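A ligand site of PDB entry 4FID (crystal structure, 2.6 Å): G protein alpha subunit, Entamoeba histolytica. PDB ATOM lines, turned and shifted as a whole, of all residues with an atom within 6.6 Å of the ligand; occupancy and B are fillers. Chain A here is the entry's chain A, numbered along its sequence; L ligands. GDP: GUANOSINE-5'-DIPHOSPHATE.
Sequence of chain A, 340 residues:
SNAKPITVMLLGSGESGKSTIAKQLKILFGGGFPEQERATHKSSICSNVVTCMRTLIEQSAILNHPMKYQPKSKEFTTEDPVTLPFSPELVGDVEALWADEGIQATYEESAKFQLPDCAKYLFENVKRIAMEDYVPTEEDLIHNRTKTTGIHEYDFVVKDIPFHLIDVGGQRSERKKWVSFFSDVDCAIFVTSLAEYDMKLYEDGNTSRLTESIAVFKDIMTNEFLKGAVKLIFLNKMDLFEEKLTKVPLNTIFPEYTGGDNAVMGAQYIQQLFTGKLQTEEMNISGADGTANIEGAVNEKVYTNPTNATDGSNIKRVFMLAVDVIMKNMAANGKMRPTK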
ATOM      1  N   GLY A  12      20.349 -24.966  18.587  1.00  0.00           N
ATOM      2  CA  GLY A  12      20.307 -23.595  18.169  1.00  0.00           C
ATOM      3  C   GLY A  12      20.070 -22.686  19.322  1.00  0.00           C
ATOM      4  O   GLY A  12      19.871 -23.163  20.414  1.00  0.00           O
ATOM      5  N   SER A  13      20.101 -21.377  19.085  1.00  0.00           N
ATOM      6  CA  SER A  13      19.648 -20.404  20.066  1.00  0.00           C
ATOM      7  C   SER A  13      18.140 -20.337  20.040  1.00  0.00           C
ATOM      8  O   SER A  13      17.475 -21.162  19.376  1.00  0.00           O
ATOM      9  CB  SER A  13      20.237 -19.028  19.769  1.00  0.00           C
ATOM     10  OG  SER A  13      21.652 -19.077  19.868  1.00  0.00           O
ATOM     11  N   GLY A  14      17.589 -19.376  20.762  1.00  0.00           N
ATOM     12  CA  GLY A  14      16.166 -19.188  20.793  1.00  0.00           C
ATOM     13  C   GLY A  14      15.695 -18.334  19.640  1.00  0.00           C
ATOM     14  O   GLY A  14      16.347 -17.339  19.279  1.00  0.00           O
ATOM     15  N   GLU A  15      14.571 -18.717  19.055  1.00  0.00           N
ATOM     16  CA  GLU A  15      13.990 -18.000  17.920  1.00  0.00           C
ATOM     17  C   GLU A  15      14.883 -18.103  16.709  1.00  0.00           C
ATOM     18  O   GLU A  15      14.966 -17.189  15.908  1.00  0.00           O
ATOM     19  CB  GLU A  15      13.734 -16.529  18.257  1.00  0.00           C
ATOM     20  CG  GLU A  15      12.320 -16.242  18.748  1.00  0.00           C
ATOM     21  CD  GLU A  15      12.292 -15.112  19.748  1.00  0.00           C
ATOM     22  OE1 GLU A  15      11.366 -14.268  19.689  1.00  0.00           O
ATOM     23  OE2 GLU A  15      13.208 -15.067  20.603  1.00  0.00           O
ATOM     24  N   SER A  16      15.555 -19.242  16.599  1.00  0.00           N
ATOM     25  CA  SER A  16      16.318 -19.553  15.415  1.00  0.00           C
ATOM     26  C   SER A  16      15.406 -20.252  14.409  1.00  0.00           C
ATOM     27  O   SER A  16      15.741 -20.399  13.229  1.00  0.00           O
ATOM     28  CB  SER A  16      17.447 -20.482  15.787  1.00  0.00           C
ATOM     29  OG  SER A  16      16.962 -21.503  16.626  1.00  0.00           O
ATOM     30  N   GLY A  17      14.236 -20.680  14.877  1.00  0.00           N
ATOM     31  CA  GLY A  17      13.309 -21.461  14.091  1.00  0.00           C
ATOM     32  C   GLY A  17      13.627 -22.941  14.054  1.00  0.00           C
ATOM     33  O   GLY A  17      13.125 -23.658  13.195  1.00  0.00           O
ATOM     34  N   LYS A  18      14.431 -23.445  14.985  1.00  0.00           N
ATOM     35  CA  LYS A  18      14.810 -24.857  14.935  1.00  0.00           C
ATOM     36  C   LYS A  18      13.632 -25.775  15.240  1.00  0.00           C
ATOM     37  O   LYS A  18      13.541 -26.900  14.722  1.00  0.00           O
ATOM     38  CB  LYS A  18      16.014 -25.158  15.843  1.00  0.00           C
ATOM     39  CG  LYS A  18      15.735 -25.912  17.104  1.00  0.00           C
ATOM     40  CD  LYS A  18      16.995 -25.912  18.011  1.00  0.00           C
ATOM     41  CE  LYS A  18      16.661 -25.480  19.440  1.00  0.00           C
ATOM     42  NZ  LYS A  18      15.246 -25.848  19.795  1.00  0.00           N
ATOM     43  N   SER A  19      12.706 -25.273  16.052  1.00  0.00           N
ATOM     44  CA  SER A  19      11.482 -26.017  16.385  1.00  0.00           C
ATOM     45  C   SER A  19      10.538 -26.073  15.172  1.00  0.00           C
ATOM     46  O   SER A  19       9.847 -27.064  14.956  1.00  0.00           O
ATOM     47  CB  SER A  19      10.805 -25.418  17.620  1.00  0.00           C
ATOM     48  OG  SER A  19       9.419 -25.172  17.405  1.00  0.00           O
ATOM     49  N   THR A  20      10.543 -25.029  14.364  1.00  0.00           N
ATOM     50  CA  THR A  20       9.788 -25.031  13.134  1.00  0.00           C
ATOM     51  C   THR A  20      10.358 -26.032  12.124  1.00  0.00           C
ATOM     52  O   THR A  20       9.630 -26.715  11.410  1.00  0.00           O
ATOM     53  CB  THR A  20       9.812 -23.672  12.473  1.00  0.00           C
ATOM     54  OG1 THR A  20       9.306 -22.688  13.406  1.00  0.00           O
ATOM     55  CG2 THR A  20       8.960 -23.709  11.192  1.00  0.00           C
ATOM     56  N   ILE A  21      11.676 -26.126  12.078  1.00  0.00           N
ATOM     57  CA  ILE A  21      12.291 -27.140  11.237  1.00  0.00           C
ATOM     58  C   ILE A  21      11.834 -28.550  11.647  1.00  0.00           C
ATOM     59  O   ILE A  21      11.544 -29.385  10.798  1.00  0.00           O
ATOM     60  CB  ILE A  21      13.808 -27.057  11.321  1.00  0.00           C
ATOM     61  CG1 ILE A  21      14.292 -25.658  10.926  1.00  0.00           C
ATOM     62  CG2 ILE A  21      14.443 -28.172  10.501  1.00  0.00           C
ATOM     63  CD1 ILE A  21      14.185 -25.364   9.466  1.00  0.00           C
ATOM     64  N   LYS A  23       9.055 -29.562  13.297  1.00  0.00           N
ATOM     65  CA  LYS A  23       7.672 -29.811  12.935  1.00  0.00           C
ATOM     66  C   LYS A  23       7.552 -30.052  11.423  1.00  0.00           C
ATOM     67  O   LYS A  23       6.787 -30.876  10.957  1.00  0.00           O
ATOM     68  CB  LYS A  23       6.777 -28.650  13.349  1.00  0.00           C
ATOM     69  CG  LYS A  23       6.346 -28.682  14.789  1.00  0.00           C
ATOM     70  CD  LYS A  23       5.733 -27.378  15.199  1.00  0.00           C
ATOM     71  CE  LYS A  23       5.596 -27.296  16.716  1.00  0.00           C
ATOM     72  NZ  LYS A  23       5.684 -25.881  17.191  1.00  0.00           N
ATOM     73  N   PRO A 116       6.212 -10.812  17.295  1.00  0.00           N
ATOM     74  CA  PRO A 116       6.390 -12.204  16.839  1.00  0.00           C
ATOM     75  C   PRO A 116       6.260 -12.334  15.318  1.00  0.00           C
ATOM     76  O   PRO A 116       5.439 -11.661  14.702  1.00  0.00           O
ATOM     77  CB  PRO A 116       5.248 -12.943  17.555  1.00  0.00           C
ATOM     78  CG  PRO A 116       4.931 -12.092  18.765  1.00  0.00           C
ATOM     79  CD  PRO A 116       5.167 -10.669  18.319  1.00  0.00           C
ATOM     80  N   ASP A 117       7.081 -13.183  14.714  1.00  0.00           N
ATOM     81  CA  ASP A 117       7.080 -13.397  13.261  1.00  0.00           C
ATOM     82  C   ASP A 117       5.712 -13.794  12.696  1.00  0.00           C
ATOM     83  O   ASP A 117       5.428 -13.564  11.523  1.00  0.00           O
ATOM     84  CB  ASP A 117       8.099 -14.486  12.869  1.00  0.00           C
ATOM     85  CG  ASP A 117       9.557 -14.093  13.164  1.00  0.00           C
ATOM     86  OD1 ASP A 117      10.465 -14.914  12.898  1.00  0.00           O
ATOM     87  OD2 ASP A 117       9.802 -12.972  13.664  1.00  0.00           O
ATOM     88  N   CYS A 118       4.879 -14.397  13.540  1.00  0.00           N
ATOM     89  CA  CYS A 118       3.648 -14.999  13.065  1.00  0.00           C
ATOM     90  C   CYS A 118       2.495 -13.995  12.934  1.00  0.00           C
ATOM     91  O   CYS A 118       1.375 -14.372  12.555  1.00  0.00           O
ATOM     92  CB  CYS A 118       3.235 -16.138  13.997  1.00  0.00           C
ATOM     93  SG  CYS A 118       2.879 -15.564  15.669  1.00  0.00           S
ATOM     94  N   LEU A 141       0.319 -24.617  12.817  1.00  0.00           N
ATOM     95  CA  LEU A 141       1.344 -25.040  13.770  1.00  0.00           C
ATOM     96  C   LEU A 141       2.738 -24.648  13.299  1.00  0.00           C
ATOM     97  O   LEU A 141       3.613 -24.369  14.140  1.00  0.00           O
ATOM     98  CB  LEU A 141       1.296 -26.554  13.997  1.00  0.00           C
ATOM     99  CG  LEU A 141       0.530 -27.154  15.182  1.00  0.00           C
ATOM    100  CD1 LEU A 141      -0.878 -26.569  15.307  1.00  0.00           C
ATOM    101  CD2 LEU A 141       0.490 -28.700  15.068  1.00  0.00           C
ATOM    102  N   ILE A 142       2.956 -24.640  11.983  1.00  0.00           N
ATOM    103  CA  ILE A 142       4.228 -24.220  11.414  1.00  0.00           C
ATOM    104  C   ILE A 142       4.493 -22.759  11.749  1.00  0.00           C
ATOM    105  O   ILE A 142       5.607 -22.380  12.121  1.00  0.00           O
ATOM    106  CB  ILE A 142       4.269 -24.360   9.874  1.00  0.00           C
ATOM    107  CG1 ILE A 142       4.331 -25.844   9.446  1.00  0.00           C
ATOM    108  CG2 ILE A 142       5.421 -23.517   9.259  1.00  0.00           C
ATOM    109  CD1 ILE A 142       5.484 -26.570  10.028  1.00  0.00           C
ATOM    110  N   HIS A 143       3.456 -21.936  11.628  1.00  0.00           N
ATOM    111  CA  HIS A 143       3.621 -20.481  11.747  1.00  0.00           C
ATOM    112  C   HIS A 143       3.470 -19.956  13.154  1.00  0.00           C
ATOM    113  O   HIS A 143       3.871 -18.827  13.447  1.00  0.00           O
ATOM    114  CB  HIS A 143       2.645 -19.744  10.841  1.00  0.00           C
ATOM    115  CG  HIS A 143       3.002 -19.802   9.401  1.00  0.00           C
ATOM    116  ND1 HIS A 143       2.585 -20.832   8.582  1.00  0.00           N
ATOM    117  CD2 HIS A 143       3.736 -18.968   8.632  1.00  0.00           C
ATOM    118  CE1 HIS A 143       3.050 -20.625   7.360  1.00  0.00           C
ATOM    119  NE2 HIS A 143       3.751 -19.507   7.365  1.00  0.00           N
ATOM    120  N   ASN A 144       2.886 -20.741  14.045  1.00  0.00           N
ATOM    121  CA  ASN A 144       2.653 -20.217  15.367  1.00  0.00           C
ATOM    122  C   ASN A 144       3.867 -20.315  16.265  1.00  0.00           C
ATOM    123  O   ASN A 144       4.654 -21.247  16.189  1.00  0.00           O
ATOM    124  CB  ASN A 144       1.460 -20.879  16.036  1.00  0.00           C
ATOM    125  CG  ASN A 144       0.991 -20.092  17.232  1.00  0.00           C
ATOM    126  OD1 ASN A 144       0.730 -18.895  17.110  1.00  0.00           O
ATOM    127  ND2 ASN A 144       0.898 -20.753  18.404  1.00  0.00           N
ATOM    128  N   ARG A 145       3.997 -19.327  17.147  1.00  0.00           N
ATOM    129  CA  ARG A 145       5.082 -19.316  18.103  1.00  0.00           C
ATOM    130  C   ARG A 145       4.779 -20.227  19.287  1.00  0.00           C
ATOM    131  O   ARG A 145       3.755 -20.072  19.955  1.00  0.00           O
ATOM    132  CB  ARG A 145       5.332 -17.875  18.542  1.00  0.00           C
ATOM    133  CG  ARG A 145       5.348 -16.896  17.365  1.00  0.00           C
ATOM    134  CD  ARG A 145       6.364 -15.771  17.567  1.00  0.00           C
ATOM    135  NE  ARG A 145       7.600 -15.954  16.807  1.00  0.00           N
ATOM    136  CZ  ARG A 145       8.694 -15.226  16.993  1.00  0.00           C
ATOM    137  NH1 ARG A 145       8.707 -14.256  17.910  1.00  0.00           N
ATOM    138  NH2 ARG A 145       9.793 -15.452  16.270  1.00  0.00           N
ATOM    139  N   THR A 146       5.650 -21.203  19.534  1.00  0.00           N
ATOM    140  CA  THR A 146       5.595 -21.976  20.788  1.00  0.00           C
ATOM    141  C   THR A 146       6.964 -22.065  21.441  1.00  0.00           C
ATOM    142  O   THR A 146       7.989 -22.007  20.760  1.00  0.00           O
ATOM    143  CB  THR A 146       5.051 -23.421  20.587  1.00  0.00           C
ATOM    144  OG1 THR A 146       5.762 -24.052  19.522  1.00  0.00           O
ATOM    145  CG2 THR A 146       3.568 -23.397  20.280  1.00  0.00           C
ATOM    146  N   LYS A 147       6.970 -22.192  22.758  1.00  0.00           N
ATOM    147  CA  LYS A 147       8.195 -22.400  23.525  1.00  0.00           C
ATOM    148  C   LYS A 147       8.438 -23.884  23.744  1.00  0.00           C
ATOM    149  O   LYS A 147       7.780 -24.499  24.578  1.00  0.00           O
ATOM    150  CB  LYS A 147       8.100 -21.714  24.884  1.00  0.00           C
ATOM    151  CG  LYS A 147       7.922 -20.218  24.832  1.00  0.00           C
ATOM    152  CD  LYS A 147       7.698 -19.670  26.234  1.00  0.00           C
ATOM    153  CE  LYS A 147       7.396 -18.188  26.209  1.00  0.00           C
ATOM    154  NZ  LYS A 147       6.961 -17.700  27.551  1.00  0.00           N
ATOM    155  N   THR A 148       9.378 -24.469  23.016  1.00  0.00           N
ATOM    156  CA  THR A 148       9.703 -25.878  23.261  1.00  0.00           C
ATOM    157  C   THR A 148      10.764 -26.011  24.353  1.00  0.00           C
ATOM    158  O   THR A 148      11.958 -26.022  24.066  1.00  0.00           O
ATOM    159  CB  THR A 148      10.111 -26.653  21.957  1.00  0.00           C
ATOM    160  OG1 THR A 148      11.462 -26.361  21.589  1.00  0.00           O
ATOM    161  CG2 THR A 148       9.162 -26.336  20.803  1.00  0.00           C
ATOM    162  N   ASP A 167      15.568 -33.087  19.137  1.00  0.00           N
ATOM    163  CA  ASP A 167      15.432 -31.622  19.171  1.00  0.00           C
ATOM    164  C   ASP A 167      15.763 -31.111  20.575  1.00  0.00           C
ATOM    165  O   ASP A 167      14.985 -31.283  21.513  1.00  0.00           O
ATOM    166  CB  ASP A 167      14.018 -31.216  18.748  1.00  0.00           C
ATOM    167  CG  ASP A 167      13.754 -29.722  18.856  1.00  0.00           C
ATOM    168  OD1 ASP A 167      12.591 -29.334  18.689  1.00  0.00           O
ATOM    169  OD2 ASP A 167      14.705 -28.935  19.101  1.00  0.00           O
ATOM    170  N   ASN A 236      18.764 -19.742   8.933  1.00  0.00           N
ATOM    171  CA  ASN A 236      17.317 -19.758   8.790  1.00  0.00           C
ATOM    172  C   ASN A 236      16.706 -18.361   8.710  1.00  0.00           C
ATOM    173  O   ASN A 236      17.353 -17.355   9.091  1.00  0.00           O
ATOM    174  CB  ASN A 236      16.695 -20.523   9.947  1.00  0.00           C
ATOM    175  CG  ASN A 236      15.262 -20.895   9.695  1.00  0.00           C
ATOM    176  OD1 ASN A 236      14.912 -21.299   8.582  1.00  0.00           O
ATOM    177  ND2 ASN A 236      14.421 -20.775  10.724  1.00  0.00           N
ATOM    178  N   LYS A 237      15.486 -18.315   8.193  1.00  0.00           N
ATOM    179  CA  LYS A 237      14.747 -17.060   8.038  1.00  0.00           C
ATOM    180  C   LYS A 237      15.342 -16.191   6.956  1.00  0.00           C
ATOM    181  O   LYS A 237      15.384 -14.975   7.096  1.00  0.00           O
ATOM    182  CB  LYS A 237      14.636 -16.302   9.362  1.00  0.00           C
ATOM    183  CG  LYS A 237      14.033 -17.167  10.503  1.00  0.00           C
ATOM    184  CD  LYS A 237      13.709 -16.317  11.729  1.00  0.00           C
ATOM    185  CE  LYS A 237      12.932 -17.107  12.765  1.00  0.00           C
ATOM    186  NZ  LYS A 237      12.671 -16.289  13.986  1.00  0.00           N
ATOM    187  N   MET A 238      15.791 -16.831   5.874  1.00  0.00           N
ATOM    188  CA  MET A 238      16.367 -16.106   4.757  1.00  0.00           C
ATOM    189  C   MET A 238      15.347 -15.121   4.153  1.00  0.00           C
ATOM    190  O   MET A 238      15.713 -14.006   3.732  1.00  0.00           O
ATOM    191  CB  MET A 238      16.912 -17.082   3.697  1.00  0.00           C
ATOM    192  CG  MET A 238      17.479 -16.413   2.434  1.00  0.00           C
ATOM    193  SD  MET A 238      19.247 -15.552   2.586  1.00  0.00           S
ATOM    194  CE  MET A 238      19.548 -15.140   0.690  1.00  0.00           C
ATOM    195  N   ASP A 239      14.089 -15.502   4.150  1.00  0.00           N
ATOM    196  CA  ASP A 239      13.015 -14.600   3.690  1.00  0.00           C
ATOM    197  C   ASP A 239      12.962 -13.303   4.509  1.00  0.00           C
ATOM    198  O   ASP A 239      12.990 -12.192   3.945  1.00  0.00           O
ATOM    199  CB  ASP A 239      11.626 -15.309   3.676  1.00  0.00           C
ATOM    200  CG  ASP A 239      11.295 -16.047   5.005  1.00  0.00           C
ATOM    201  OD1 ASP A 239      12.218 -16.584   5.686  1.00  0.00           O
ATOM    202  OD2 ASP A 239      10.089 -16.108   5.360  1.00  0.00           O
ATOM    203  N   LEU A 240      12.914 -13.454   5.841  1.00  0.00           N
ATOM    204  CA  LEU A 240      12.838 -12.333   6.767  1.00  0.00           C
ATOM    205  C   LEU A 240      14.073 -11.472   6.643  1.00  0.00           C
ATOM    206  O   LEU A 240      14.007 -10.248   6.719  1.00  0.00           O
ATOM    207  CB  LEU A 240      12.688 -12.811   8.211  1.00  0.00           C
ATOM    208  CG  LEU A 240      11.341 -13.495   8.474  1.00  0.00           C
ATOM    209  CD1 LEU A 240      11.193 -13.928   9.949  1.00  0.00           C
ATOM    210  CD2 LEU A 240      10.192 -12.565   8.052  1.00  0.00           C
ATOM    211  N   THR A 307      17.966 -21.334   4.782  1.00  0.00           N
ATOM    212  CA  THR A 307      16.664 -21.954   4.797  1.00  0.00           C
ATOM    213  C   THR A 307      15.530 -20.983   5.127  1.00  0.00           C
ATOM    214  O   THR A 307      15.717 -19.891   5.733  1.00  0.00           O
ATOM    215  CB  THR A 307      16.621 -23.129   5.806  1.00  0.00           C
ATOM    216  OG1 THR A 307      16.601 -22.619   7.142  1.00  0.00           O
ATOM    217  CG2 THR A 307      17.823 -24.028   5.639  1.00  0.00           C
ATOM    218  N   ASN A 308      14.343 -21.397   4.701  1.00  0.00           N
ATOM    219  CA  ASN A 308      13.108 -20.746   5.081  1.00  0.00           C
ATOM    220  C   ASN A 308      12.177 -21.821   5.664  1.00  0.00           C
ATOM    221  O   ASN A 308      11.424 -22.487   4.948  1.00  0.00           O
ATOM    222  CB  ASN A 308      12.493 -19.973   3.904  1.00  0.00           C
ATOM    223  CG  ASN A 308      11.120 -19.395   4.219  1.00  0.00           C
ATOM    224  OD1 ASN A 308      10.658 -19.416   5.377  1.00  0.00           O
ATOM    225  ND2 ASN A 308      10.442 -18.861   3.189  1.00  0.00           N
ATOM    226  N   ALA A 309      12.285 -21.993   6.983  1.00  0.00           N
ATOM    227  CA  ALA A 309      11.586 -23.036   7.729  1.00  0.00           C
ATOM    228  C   ALA A 309      10.039 -23.048   7.605  1.00  0.00           C
ATOM    229  O   ALA A 309       9.403 -24.078   7.862  1.00  0.00           O
ATOM    230  CB  ALA A 309      11.998 -22.986   9.203  1.00  0.00           C
ATOM    231  N   THR A 310       9.431 -21.938   7.247  1.00  0.00           N
ATOM    232  CA  THR A 310       7.977 -21.896   7.095  1.00  0.00           C
ATOM    233  C   THR A 310       7.557 -22.297   5.684  1.00  0.00           C
ATOM    234  O   THR A 310       6.384 -22.214   5.343  1.00  0.00           O
ATOM    235  CB  THR A 310       7.414 -20.506   7.391  1.00  0.00           C
ATOM    236  OG1 THR A 310       8.003 -19.557   6.502  1.00  0.00           O
ATOM    237  CG2 THR A 310       7.729 -20.115   8.818  1.00  0.00           C
ATOM    238  N   ASP A 311       8.524 -22.761   4.886  1.00  0.00           N
ATOM    239  CA  ASP A 311       8.298 -23.180   3.501  1.00  0.00           C
ATOM    240  C   ASP A 311       8.613 -24.673   3.319  1.00  0.00           C
ATOM    241  O   ASP A 311       9.772 -25.050   3.133  1.00  0.00           O
ATOM    242  CB  ASP A 311       9.175 -22.331   2.576  1.00  0.00           C
ATOM    243  CG  ASP A 311       9.058 -22.736   1.121  1.00  0.00           C
ATOM    244  OD1 ASP A 311       8.553 -23.849   0.829  1.00  0.00           O
ATOM    245  OD2 ASP A 311       9.493 -21.930   0.264  1.00  0.00           O
HETATM  246  PB  GDP L   1      12.912 -22.439  18.746  1.00  0.00           P
HETATM  247  O1B GDP L   1      11.867 -23.278  19.443  1.00  0.00           O
HETATM  248  O2B GDP L   1      13.608 -21.573  19.766  1.00  0.00           O
HETATM  249  O3B GDP L   1      13.901 -23.393  18.123  1.00  0.00           O
HETATM  250  O3A GDP L   1      12.280 -21.478  17.595  1.00  0.00           O
HETATM  251  PA  GDP L   1      10.775 -21.636  16.982  1.00  0.00           P
HETATM  252  O1A GDP L   1      10.699 -22.775  15.998  1.00  0.00           O
HETATM  253  O2A GDP L   1       9.743 -21.814  18.080  1.00  0.00           O
HETATM  254  O5' GDP L   1      10.514 -20.213  16.248  1.00  0.00           O
HETATM  255  C5' GDP L   1       9.391 -19.400  16.632  1.00  0.00           C
HETATM  256  C4' GDP L   1       8.822 -18.596  15.462  1.00  0.00           C
HETATM  257  O4' GDP L   1       9.759 -18.439  14.383  1.00  0.00           O
HETATM  258  C3' GDP L   1       7.556 -19.222  14.872  1.00  0.00           C
HETATM  259  O3' GDP L   1       6.478 -18.271  14.911  1.00  0.00           O
HETATM  260  C2' GDP L   1       7.941 -19.601  13.443  1.00  0.00           C
HETATM  261  O2' GDP L   1       6.813 -19.477  12.549  1.00  0.00           O
HETATM  262  C1' GDP L   1       9.079 -18.634  13.135  1.00  0.00           C
HETATM  263  N9  GDP L   1       9.994 -19.121  12.067  1.00  0.00           N
HETATM  264  C8  GDP L   1      10.886 -20.144  12.125  1.00  0.00           C
HETATM  265  N7  GDP L   1      11.551 -20.292  10.949  1.00  0.00           N
HETATM  266  C5  GDP L   1      11.089 -19.343  10.101  1.00  0.00           C
HETATM  267  C6  GDP L   1      11.343 -18.928   8.701  1.00  0.00           C
HETATM  268  O6  GDP L   1      12.183 -19.510   7.991  1.00  0.00           O
HETATM  269  N1  GDP L   1      10.646 -17.902   8.201  1.00  0.00           N
HETATM  270  C2  GDP L   1       9.731 -17.229   8.937  1.00  0.00           C
HETATM  271  N2  GDP L   1       9.081 -16.195   8.369  1.00  0.00           N
HETATM  272  N3  GDP L   1       9.445 -17.551  10.230  1.00  0.00           N
HETATM  273  C4  GDP L   1      10.081 -18.576  10.849  1.00  0.00           C
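O2' of the ligand is in hydrogen-bond range of O of Ile 142.
The side-chain amide nitrogen (ND2) of Asn 236 is in hydrogen-bond range of a nitrogen (N7) of the ligand (2.9 Å).
The side-chain carboxylate of Asp 239 lies within hydrogen-bond range of a nitrogen (N2) of the ligand, at 3.2 Å.
OG1 of Thr 20 lies within hydrogen-bond range of O1A of the ligand.
The backbone NH of Ser 19 is in hydrogen-bond range of an oxygen (O3B) of the ligand, at 3.0 Å.
An oxygen (O3B) of the ligand sits at hydrogen-bond distance from the backbone NH (N) of Lys 18 (3.2 Å).
The backbone carbonyl oxygen (O) of His 143 sits at hydrogen-bond distance from an oxygen (O3') of the ligand.
O6 of the ligand sits close to OD1 of Asn 308 (3.0 Å).
N of Gly 17 is in hydrogen-bond range of O3A of the ligand, 3.4 Å away.
NE of Arg 145 sits close to O3' of the ligand, 3.2 Å away.
An oxygen (O1A) of the ligand sits at hydrogen-bond distance from the side-chain hydroxyl (OG) of Ser 19, at 3.1 Å.
An oxygen (O3B) of the ligand lies within salt-bridge range of the side-chain amino group (NZ) of Lys 18 (3.3 Å).
O2B of the ligand is in hydrogen-bond range of N of Glu 15, 3.1 Å away.
N of Thr 20 lies within hydrogen-bond range of O1A of the ligand.
An oxygen (O6) of the ligand lies within hydrogen-bond range of the backbone NH (N) of Ala 309, at 2.7 Å.
O of Glu 15 sits at hydrogen-bond distance from NZ of Lys 237.
OD1 of Asn 236 lies within hydrogen-bond range of OG1 of Thr 307.
The side-chain amino group (NZ) of Lys 18 lies within salt-bridge range of the side-chain carboxylate (OD2) of Asp 167, 3.2 Å away.
The side-chain amide oxygen (OD1) of Asn 308 is in hydrogen-bond range of the side-chain hydroxyl (OG1) of Thr 310 (2.9 Å).
The side-chain carboxylate of Asp 117 is in salt-bridge range of the side-chain amino group of Lys 237 (2.8 Å).
The side-chain hydroxyl of Ser 16 is in hydrogen-bond range of the backbone carbonyl oxygen of Ser 13, at 2.8 Å.
O of Ser 16 sits at hydrogen-bond distance from ND2 of Asn 236 (2.9 Å).
The side-chain amino group (NZ) of Lys 23 sits at hydrogen-bond distance from the side-chain hydroxyl (OG1) of Thr 146 (3.0 Å).
The backbone carbonyl oxygen (O) of Thr 146 sits close to an oxygen (O2A) of the ligand (3.2 Å).
Residues that only touch the ligand: Thr 310 (3.4 Å), Leu 240 (3.5 Å), Lys 237 (3.5 Å), Asn 144 (3.6 Å), Gly 14 (3.6 Å), Thr 148 (3.8 Å), Asp 117 (3.9 Å), Ser 16 (3.9 Å), Ser 13 (3.9 Å) and Cys 118 (3.99 Å).
Hydrophobic or aromatic side chains within 4 Å of the ligand: Leu 240 and Ala 309.
23 residues have an atom within 4 Å of the ligand: Ser 13, Gly 14, Glu 15, Ser 16, Gly 17, Lys 18, Ser 19, Thr 20, Asp 117, Cys 118, Ile 142, His 143, Asn 144, Arg 145, Thr 146, Thr 148, Asn 236, Lys 237, Asp 239, Leu 240, Asn 308, Ala 309 and Thr 310.
The nearest printed residue that does not touch the ligand is Thr 307 (4.2 Å).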
